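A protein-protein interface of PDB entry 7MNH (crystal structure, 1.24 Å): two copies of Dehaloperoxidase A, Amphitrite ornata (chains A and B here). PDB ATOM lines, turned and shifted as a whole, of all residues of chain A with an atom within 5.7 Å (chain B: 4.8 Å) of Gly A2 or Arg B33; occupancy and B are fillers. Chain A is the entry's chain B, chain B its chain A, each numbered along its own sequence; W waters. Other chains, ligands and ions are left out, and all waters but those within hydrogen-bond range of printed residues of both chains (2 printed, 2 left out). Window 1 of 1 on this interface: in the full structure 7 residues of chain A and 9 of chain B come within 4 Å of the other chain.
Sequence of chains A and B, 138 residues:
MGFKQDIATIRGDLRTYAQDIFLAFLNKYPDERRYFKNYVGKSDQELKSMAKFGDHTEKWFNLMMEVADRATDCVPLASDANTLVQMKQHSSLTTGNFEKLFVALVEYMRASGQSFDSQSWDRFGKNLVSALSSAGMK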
ATOM      1  N   GLY A   2      -1.091 -15.546 -30.911  1.00  0.00           N
ATOM      2  CA  GLY A   2      -1.744 -16.623 -30.171  1.00  0.00           C
ATOM      3  C   GLY A   2      -1.684 -17.937 -30.923  1.00  0.00           C
ATOM      4  O   GLY A   2      -0.891 -18.067 -31.846  1.00  0.00           O
ATOM      5  N   PHE A   3      -2.485 -18.890 -30.485  1.00  0.00           N
ATOM      6  CA  PHE A   3      -2.430 -20.258 -31.046  1.00  0.00           C
ATOM      7  C   PHE A   3      -2.750 -20.248 -32.540  1.00  0.00           C
ATOM      8  O   PHE A   3      -2.057 -20.856 -33.355  1.00  0.00           O
ATOM      9  CB  PHE A   3      -3.432 -21.100 -30.264  1.00  0.00           C
ATOM     10  CG  PHE A   3      -3.493 -22.555 -30.665  1.00  0.00           C
ATOM     11  CD1 PHE A   3      -2.472 -23.426 -30.294  1.00  0.00           C
ATOM     12  CD2 PHE A   3      -4.568 -23.056 -31.362  1.00  0.00           C
ATOM     13  CE1 PHE A   3      -2.582 -24.771 -30.584  1.00  0.00           C
ATOM     14  CE2 PHE A   3      -4.662 -24.404 -31.638  1.00  0.00           C
ATOM     15  CZ  PHE A   3      -3.667 -25.247 -31.259  1.00  0.00           C
ATOM     16  N   LYS A   4      -3.821 -19.557 -32.928  1.00  0.00           N
ATOM     17  CA  LYS A   4      -4.247 -19.544 -34.330  1.00  0.00           C
ATOM     18  C   LYS A   4      -3.141 -18.955 -35.203  1.00  0.00           C
ATOM     19  O   LYS A   4      -2.831 -19.471 -36.279  1.00  0.00           O
ATOM     20  CB  LYS A   4      -5.556 -18.775 -34.455  1.00  0.00           C
ATOM     21  CG  LYS A   4      -6.799 -19.633 -34.470  1.00  0.00           C
ATOM     22  CD  LYS A   4      -6.815 -20.645 -35.614  1.00  0.00           C
ATOM     23  CE  LYS A   4      -8.062 -20.732 -36.432  1.00  0.00           C
ATOM     24  NZ  LYS A   4      -8.408 -22.157 -36.432  1.00  0.00           N
ATOM     25  N   GLN A   5      -2.526 -17.859 -34.775  1.00  0.00           N
ATOM     26  CA  GLN A   5      -1.449 -17.243 -35.563  1.00  0.00           C
ATOM     27  C   GLN A   5      -0.218 -18.184 -35.561  1.00  0.00           C
ATOM     28  O   GLN A   5       0.478 -18.269 -36.585  1.00  0.00           O
ATOM     29  CB  GLN A   5      -1.116 -15.833 -35.080  1.00  0.00           C
ATOM     30  CG  GLN A   5      -0.017 -15.173 -35.922  1.00  0.00           C
ATOM     31  CD  GLN A   5      -0.426 -15.017 -37.364  1.00  0.00           C
ATOM     32  OE1 GLN A   5      -1.597 -14.914 -37.728  1.00  0.00           O
ATOM     33  NE2 GLN A   5       0.541 -15.020 -38.277  1.00  0.00           N
ATOM     34  N   ASP A   6       0.067 -18.860 -34.445  1.00  0.00           N
ATOM     35  CA  ASP A   6       1.204 -19.812 -34.408  1.00  0.00           C
ATOM     36  C   ASP A   6       1.047 -20.888 -35.480  1.00  0.00           C
ATOM     37  O   ASP A   6       2.062 -21.292 -36.058  1.00  0.00           O
ATOM     38  CB  ASP A   6       1.294 -20.487 -33.067  1.00  0.00           C
ATOM     39  CG  ASP A   6       1.748 -19.615 -31.911  1.00  0.00           C
ATOM     40  OD1 ASP A   6       2.273 -18.491 -32.157  1.00  0.00           O
ATOM     41  OD2 ASP A   6       1.590 -20.079 -30.772  1.00  0.00           O
ATOM     42  N   ILE A   7      -0.168 -21.334 -35.768  1.00  0.00           N
ATOM     43  CA  ILE A   7      -0.376 -22.338 -36.829  1.00  0.00           C
ATOM     44  C   ILE A   7       0.109 -21.745 -38.148  1.00  0.00           C
ATOM     45  O   ILE A   7       0.776 -22.425 -38.932  1.00  0.00           O
ATOM     46  CB  ILE A   7      -1.853 -22.719 -36.900  1.00  0.00           C
ATOM     47  CG1 ILE A   7      -2.306 -23.395 -35.607  1.00  0.00           C
ATOM     48  CG2 ILE A   7      -2.098 -23.570 -38.140  1.00  0.00           C
ATOM     49  CD1 ILE A   7      -3.801 -23.586 -35.472  1.00  0.00           C
ATOM     50  N   ASP A 117       2.780 -18.916 -28.540  1.00  0.00           N
ATOM     51  CA  ASP A 117       1.922 -19.019 -27.352  1.00  0.00           C
ATOM     52  C   ASP A 117       2.092 -20.432 -26.796  1.00  0.00           C
ATOM     53  O   ASP A 117       1.232 -21.323 -26.937  1.00  0.00           O
ATOM     54  CB  ASP A 117       0.480 -18.693 -27.693  1.00  0.00           C
ATOM     55  CG  ASP A 117      -0.515 -18.792 -26.565  1.00  0.00           C
ATOM     56  OD1 ASP A 117      -0.059 -18.993 -25.421  1.00  0.00           O
ATOM     57  OD2 ASP A 117      -1.706 -18.658 -26.856  1.00  0.00           O
ATOM     58  N   TRP A 121      -0.113 -24.257 -26.710  1.00  0.00           N
ATOM     59  CA  TRP A 121       0.344 -25.542 -27.286  1.00  0.00           C
ATOM     60  C   TRP A 121       0.353 -26.617 -26.218  1.00  0.00           C
ATOM     61  O   TRP A 121       0.023 -27.769 -26.495  1.00  0.00           O
ATOM     62  CB  TRP A 121       1.682 -25.411 -28.032  1.00  0.00           C
ATOM     63  CG  TRP A 121       1.488 -24.635 -29.280  1.00  0.00           C
ATOM     64  CD1 TRP A 121       1.547 -23.288 -29.446  1.00  0.00           C
ATOM     65  CD2 TRP A 121       0.975 -25.136 -30.524  1.00  0.00           C
ATOM     66  NE1 TRP A 121       1.183 -22.929 -30.714  1.00  0.00           N
ATOM     67  CE2 TRP A 121       0.816 -24.054 -31.400  1.00  0.00           C
ATOM     68  CE3 TRP A 121       0.704 -26.432 -30.969  1.00  0.00           C
ATOM     69  CZ2 TRP A 121       0.371 -24.223 -32.704  1.00  0.00           C
ATOM     70  CZ3 TRP A 121       0.226 -26.614 -32.269  1.00  0.00           C
ATOM     71  CH2 TRP A 121       0.041 -25.496 -33.099  1.00  0.00           C
ATOM     72  N   LEU B  26      -0.349  -8.674 -27.495  1.00  0.00           N
ATOM     73  CA  LEU B  26      -0.998  -9.985 -27.332  1.00  0.00           C
ATOM     74  C   LEU B  26      -0.004 -11.106 -27.546  1.00  0.00           C
ATOM     75  O   LEU B  26      -0.153 -12.182 -26.887  1.00  0.00           O
ATOM     76  CB  LEU B  26      -2.167 -10.162 -28.298  1.00  0.00           C
ATOM     77  CG  LEU B  26      -3.329  -9.176 -28.135  1.00  0.00           C
ATOM     78  CD1 LEU B  26      -4.450  -9.613 -29.060  1.00  0.00           C
ATOM     79  CD2 LEU B  26      -3.808  -9.185 -26.703  1.00  0.00           C
ATOM     80  N   ASN B  27       1.000 -10.960 -28.366  1.00  0.00           N
ATOM     81  CA  ASN B  27       1.940 -12.057 -28.590  1.00  0.00           C
ATOM     82  C   ASN B  27       2.823 -12.198 -27.374  1.00  0.00           C
ATOM     83  O   ASN B  27       3.201 -13.368 -27.048  1.00  0.00           O
ATOM     84  CB  ASN B  27       2.782 -11.813 -29.822  1.00  0.00           C
ATOM     85  CG  ASN B  27       2.002 -11.967 -31.100  1.00  0.00           C
ATOM     86  OD1 ASN B  27       0.925 -12.553 -31.122  1.00  0.00           O
ATOM     87  ND2 ASN B  27       2.524 -11.371 -32.163  1.00  0.00           N
ATOM     88  N   TYR B  29       2.047 -11.299 -24.292  1.00  0.00           N
ATOM     89  CA  TYR B  29       1.167 -11.592 -23.135  1.00  0.00           C
ATOM     90  C   TYR B  29      -0.136 -12.184 -23.624  1.00  0.00           C
ATOM     91  O   TYR B  29      -1.197 -11.549 -23.628  1.00  0.00           O
ATOM     92  CB  TYR B  29       0.880 -10.313 -22.353  1.00  0.00           C
ATOM     93  CG  TYR B  29       2.124  -9.680 -21.795  1.00  0.00           C
ATOM     94  CD1 TYR B  29       2.770 -10.209 -20.688  1.00  0.00           C
ATOM     95  CD2 TYR B  29       2.657  -8.553 -22.387  1.00  0.00           C
ATOM     96  CE1 TYR B  29       3.924  -9.619 -20.184  1.00  0.00           C
ATOM     97  CE2 TYR B  29       3.768  -7.934 -21.854  1.00  0.00           C
ATOM     98  CZ  TYR B  29       4.416  -8.467 -20.767  1.00  0.00           C
ATOM     99  OH  TYR B  29       5.540  -7.853 -20.258  1.00  0.00           O
ATOM    100  N   PRO B  30      -0.076 -13.436 -24.117  1.00  0.00           N
ATOM    101  CA  PRO B  30      -1.242 -14.005 -24.775  1.00  0.00           C
ATOM    102  C   PRO B  30      -2.486 -14.087 -23.911  1.00  0.00           C
ATOM    103  O   PRO B  30      -3.577 -14.054 -24.406  1.00  0.00           O
ATOM    104  CB  PRO B  30      -0.785 -15.416 -25.193  1.00  0.00           C
ATOM    105  CG  PRO B  30       0.446 -15.655 -24.362  1.00  0.00           C
ATOM    106  CD  PRO B  30       1.096 -14.313 -24.162  1.00  0.00           C
ATOM    107  N   ASP B  31      -2.303 -14.163 -22.603  1.00  0.00           N
ATOM    108  CA  ASP B  31      -3.459 -14.191 -21.681  1.00  0.00           C
ATOM    109  C   ASP B  31      -4.316 -12.929 -21.783  1.00  0.00           C
ATOM    110  O   ASP B  31      -5.503 -12.957 -21.473  1.00  0.00           O
ATOM    111  CB  ASP B  31      -2.991 -14.512 -20.247  1.00  0.00           C
ATOM    112  CG  ASP B  31      -2.690 -16.014 -20.079  1.00  0.00           C
ATOM    113  OD1 ASP B  31      -1.859 -16.601 -20.849  1.00  0.00           O
ATOM    114  OD2 ASP B  31      -3.355 -16.627 -19.220  1.00  0.00           O
ATOM    115  N   GLU B  32      -3.737 -11.846 -22.248  1.00  0.00           N
ATOM    116  CA  GLU B  32      -4.457 -10.549 -22.362  1.00  0.00           C
ATOM    117  C   GLU B  32      -5.557 -10.580 -23.440  1.00  0.00           C
ATOM    118  O   GLU B  32      -6.423  -9.738 -23.430  1.00  0.00           O
ATOM    119  CB  GLU B  32      -3.466  -9.427 -22.657  1.00  0.00           C
ATOM    120  CG  GLU B  32      -2.455  -9.175 -21.545  1.00  0.00           C
ATOM    121  CD  GLU B  32      -3.044  -8.672 -20.255  1.00  0.00           C
ATOM    122  OE1 GLU B  32      -3.590  -7.586 -20.268  1.00  0.00           O
ATOM    123  OE2 GLU B  32      -3.018  -9.448 -19.244  1.00  0.00           O
ATOM    124  N   ARG B  33      -5.517 -11.565 -24.339  1.00  0.00           N
ATOM    125  CA  ARG B  33      -6.543 -11.668 -25.393  1.00  0.00           C
ATOM    126  C   ARG B  33      -7.907 -11.959 -24.768  1.00  0.00           C
ATOM    127  O   ARG B  33      -8.913 -11.637 -25.390  1.00  0.00           O
ATOM    128  CB  ARG B  33      -6.145 -12.705 -26.451  1.00  0.00           C
ATOM    129  CG  ARG B  33      -7.023 -12.654 -27.694  1.00  0.00           C
ATOM    130  CD  ARG B  33      -6.613 -13.712 -28.719  1.00  0.00           C
ATOM    131  NE  ARG B  33      -5.279 -13.450 -29.222  1.00  0.00           N
ATOM    132  CZ  ARG B  33      -4.935 -13.317 -30.508  1.00  0.00           C
ATOM    133  NH1 ARG B  33      -5.858 -13.250 -31.429  1.00  0.00           N
ATOM    134  NH2 ARG B  33      -3.671 -13.126 -30.809  1.00  0.00           N
ATOM    135  N   ARG B  34      -7.958 -12.465 -23.541  1.00  0.00           N
ATOM    136  CA  ARG B  34      -9.254 -12.794 -22.923  1.00  0.00           C
ATOM    137  C   ARG B  34     -10.141 -11.558 -22.778  1.00  0.00           C
ATOM    138  O   ARG B  34     -11.346 -11.691 -22.687  1.00  0.00           O
ATOM    139  CB  ARG B  34      -9.062 -13.416 -21.547  1.00  0.00           C
ATOM    140  CG  ARG B  34      -8.549 -12.469 -20.475  1.00  0.00           C
ATOM    141  CD  ARG B  34      -8.045 -13.322 -19.312  1.00  0.00           C
ATOM    142  NE  ARG B  34      -7.667 -12.597 -18.102  1.00  0.00           N
ATOM    143  CZ  ARG B  34      -6.455 -12.144 -17.795  1.00  0.00           C
ATOM    144  NH1 ARG B  34      -5.448 -12.242 -18.653  1.00  0.00           N
ATOM    145  NH2 ARG B  34      -6.274 -11.518 -16.650  1.00  0.00           N
ATOM    146  N   TYR B  35      -9.558 -10.355 -22.751  1.00  0.00           N
ATOM    147  CA  TYR B  35     -10.356  -9.109 -22.655  1.00  0.00           C
ATOM    148  C   TYR B  35     -10.991  -8.708 -23.967  1.00  0.00           C
ATOM    149  O   TYR B  35     -11.820  -7.822 -23.980  1.00  0.00           O
ATOM    150  CB  TYR B  35      -9.466  -7.982 -22.161  1.00  0.00           C
ATOM    151  CG  TYR B  35      -8.958  -8.180 -20.769  1.00  0.00           C
ATOM    152  CD1 TYR B  35      -9.791  -8.047 -19.663  1.00  0.00           C
ATOM    153  CD2 TYR B  35      -7.650  -8.526 -20.556  1.00  0.00           C
ATOM    154  CE1 TYR B  35      -9.289  -8.199 -18.382  1.00  0.00           C
ATOM    155  CE2 TYR B  35      -7.160  -8.751 -19.294  1.00  0.00           C
ATOM    156  CZ  TYR B  35      -7.974  -8.540 -18.212  1.00  0.00           C
ATOM    157  OH  TYR B  35      -7.419  -8.747 -16.980  1.00  0.00           O
ATOM    158  N   PHE B  36     -10.699  -9.409 -25.039  1.00  0.00           N
ATOM    159  CA  PHE B  36     -11.156  -9.120 -26.411  1.00  0.00           C
ATOM    160  C   PHE B  36     -11.793 -10.395 -26.933  1.00  0.00           C
ATOM    161  O   PHE B  36     -11.213 -11.080 -27.752  1.00  0.00           O
ATOM    162  CB  PHE B  36      -9.970  -8.667 -27.259  1.00  0.00           C
ATOM    163  CG  PHE B  36      -9.185  -7.542 -26.652  1.00  0.00           C
ATOM    164  CD1 PHE B  36      -9.562  -6.232 -26.887  1.00  0.00           C
ATOM    165  CD2 PHE B  36      -8.091  -7.792 -25.858  1.00  0.00           C
ATOM    166  CE1 PHE B  36      -8.829  -5.185 -26.334  1.00  0.00           C
ATOM    167  CE2 PHE B  36      -7.355  -6.759 -25.305  1.00  0.00           C
ATOM    168  CZ  PHE B  36      -7.739  -5.456 -25.539  1.00  0.00           C
ATOM    169  N   LYS B  37     -13.010 -10.646 -26.502  1.00  0.00           N
ATOM    170  CA  LYS B  37     -13.606 -11.977 -26.716  1.00  0.00           C
ATOM    171  C   LYS B  37     -13.764 -12.256 -28.215  1.00  0.00           C
ATOM    172  O   LYS B  37     -13.754 -13.426 -28.599  1.00  0.00           O
ATOM    173  CB  LYS B  37     -14.930 -12.122 -25.983  1.00  0.00           C
ATOM    174  CG  LYS B  37     -16.043 -11.251 -26.477  1.00  0.00           C
ATOM    175  CD  LYS B  37     -17.233 -11.334 -25.554  1.00  0.00           C
ATOM    176  CE  LYS B  37     -18.456 -10.761 -26.209  1.00  0.00           C
ATOM    177  NZ  LYS B  37     -19.584 -10.608 -25.263  1.00  0.00           N
ATOM    178  N   TYR B  39     -11.721 -11.590 -30.539  1.00  0.00           N
ATOM    179  CA  TYR B  39     -10.423 -11.836 -31.226  1.00  0.00           C
ATOM    180  C   TYR B  39      -9.882 -13.233 -30.933  1.00  0.00           C
ATOM    181  O   TYR B  39      -8.851 -13.610 -31.505  1.00  0.00           O
ATOM    182  CB  TYR B  39      -9.397 -10.772 -30.847  1.00  0.00           C
ATOM    183  CG  TYR B  39      -9.790  -9.344 -31.125  1.00  0.00           C
ATOM    184  CD1 TYR B  39     -10.826  -8.961 -31.962  1.00  0.00           C
ATOM    185  CD2 TYR B  39      -9.109  -8.357 -30.446  1.00  0.00           C
ATOM    186  CE1 TYR B  39     -11.179  -7.619 -32.116  1.00  0.00           C
ATOM    187  CE2 TYR B  39      -9.441  -7.028 -30.586  1.00  0.00           C
ATOM    188  CZ  TYR B  39     -10.474  -6.677 -31.403  1.00  0.00           C
ATOM    189  OH  TYR B  39     -10.743  -5.340 -31.557  1.00  0.00           O
ATOM    190  N   VAL B  40     -10.494 -13.953 -30.017  1.00  0.00           N
ATOM    191  CA  VAL B  40     -10.037 -15.322 -29.666  1.00  0.00           C
ATOM    192  C   VAL B  40     -10.191 -16.206 -30.894  1.00  0.00           C
ATOM    193  O   VAL B  40     -11.229 -16.190 -31.553  1.00  0.00           O
ATOM    194  CB  VAL B  40     -10.871 -15.791 -28.459  1.00  0.00           C
ATOM    195  CG1 VAL B  40     -10.724 -17.286 -28.184  1.00  0.00           C
ATOM    196  CG2 VAL B  40     -10.561 -14.966 -27.210  1.00  0.00           C
ATOM    197  N   LYS B  42      -8.620 -16.259 -33.761  1.00  0.00           N
ATOM    198  CA  LYS B  42      -8.589 -15.559 -35.049  1.00  0.00           C
ATOM    199  C   LYS B  42      -7.113 -15.317 -35.375  1.00  0.00           C
ATOM    200  O   LYS B  42      -6.383 -14.767 -34.517  1.00  0.00           O
ATOM    201  CB  LYS B  42      -9.317 -14.219 -35.017  1.00  0.00           C
ATOM    202  CG  LYS B  42     -10.804 -14.233 -34.683  1.00  0.00           C
ATOM    203  CD  LYS B  42     -11.634 -14.971 -35.596  1.00  0.00           C
ATOM    204  CE  LYS B  42     -13.086 -14.719 -35.222  1.00  0.00           C
ATOM    205  NZ  LYS B  42     -14.001 -15.456 -36.122  1.00  0.00           N
ATOM    206  N   LEU B  47      -8.218 -11.086 -38.114  1.00  0.00           N
ATOM    207  CA  LEU B  47      -8.468  -9.869 -37.298  1.00  0.00           C
ATOM    208  C   LEU B  47      -8.468  -8.631 -38.189  1.00  0.00           C
ATOM    209  O   LEU B  47      -9.370  -7.799 -38.070  1.00  0.00           O
ATOM    210  CB  LEU B  47      -7.398  -9.739 -36.228  1.00  0.00           C
ATOM    211  CG  LEU B  47      -7.466 -10.782 -35.122  1.00  0.00           C
ATOM    212  CD1 LEU B  47      -6.292 -10.624 -34.187  1.00  0.00           C
ATOM    213  CD2 LEU B  47      -8.787 -10.653 -34.369  1.00  0.00           C
HETATM  214  O   HOH W   1      -1.247 -13.265 -32.770  1.00  0.00           O
HETATM  215  O   HOH W   2      -1.983 -18.600 -23.419  1.00  0.00           O
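The backbone carbonyl oxygen (O) of Tyr B39 lies within hydrogen-bond range of the guanidinium group (NH1) of Arg B33. The guanidinium group (NH1) of Arg B33 lies within hydrogen-bond range of the backbone carbonyl oxygen (O) of Lys B42 (3.5 Å). The backbone NH (N) of Asp A117 is in hydrogen-bond range of the side-chain carboxylate (OD2) of Asp A6, 2.8 Å away.
Gly A2 touches Asn B27. Gly A2 touches Arg B33 (N to NH2, 3.5 Å). Lys B42 touches Lys A4 (N to CG, 3.9 Å). Asp A117 touches Pro B30.
Of chain B, only Asn B27 and Arg B33 come within 4 Å of Gly A2. Arg B33 touches just one residue of chain A: Gly A2 (3.5 Å). Printed residues of chain A within 4 Å of Pro B30: Asp A117. Of the printed residues of chain B, Asp A117 touches Pro B30 (3.5 Å). Leu B26 touches none of the printed residues of chain A. The nearest printed residue of chain B that does not touch Gly A2 is Pro B30 (5.2 Å). The nearest printed residue of chain B that does not touch Lys A4 is Val B40 (6.0 Å).
Hydrophobic or aromatic side chains of chain B within 4 Å of the printed part of chain A: Pro B30. Along chain B the printed residues that touch a printed residue of chain A span positions 27 to 42. Of the 8 printed residues of chain A, 3 touch a printed residue of chain B. Among the printed residues, no Asp or Glu carboxylate lies within 4 Å of a Lys or Arg side-chain nitrogen of the other chain.
No position is printed for both chains. Of the 4 pairs that touch across the chains among the printed residues, none has its exchanged pair printed and touching as well.
Water W2 lies within hydrogen-bond range of the side-chain carboxylate of Asp A117 (2.8 Å) and the side-chain carboxylate of Asp B31 (3.3 Å). Water W1 lies within hydrogen-bond range of the side-chain amide oxygen (OD1) of Asn B27, the backbone NH (N) of Gly A2 and the guanidinium group (NH2) of Arg B33.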
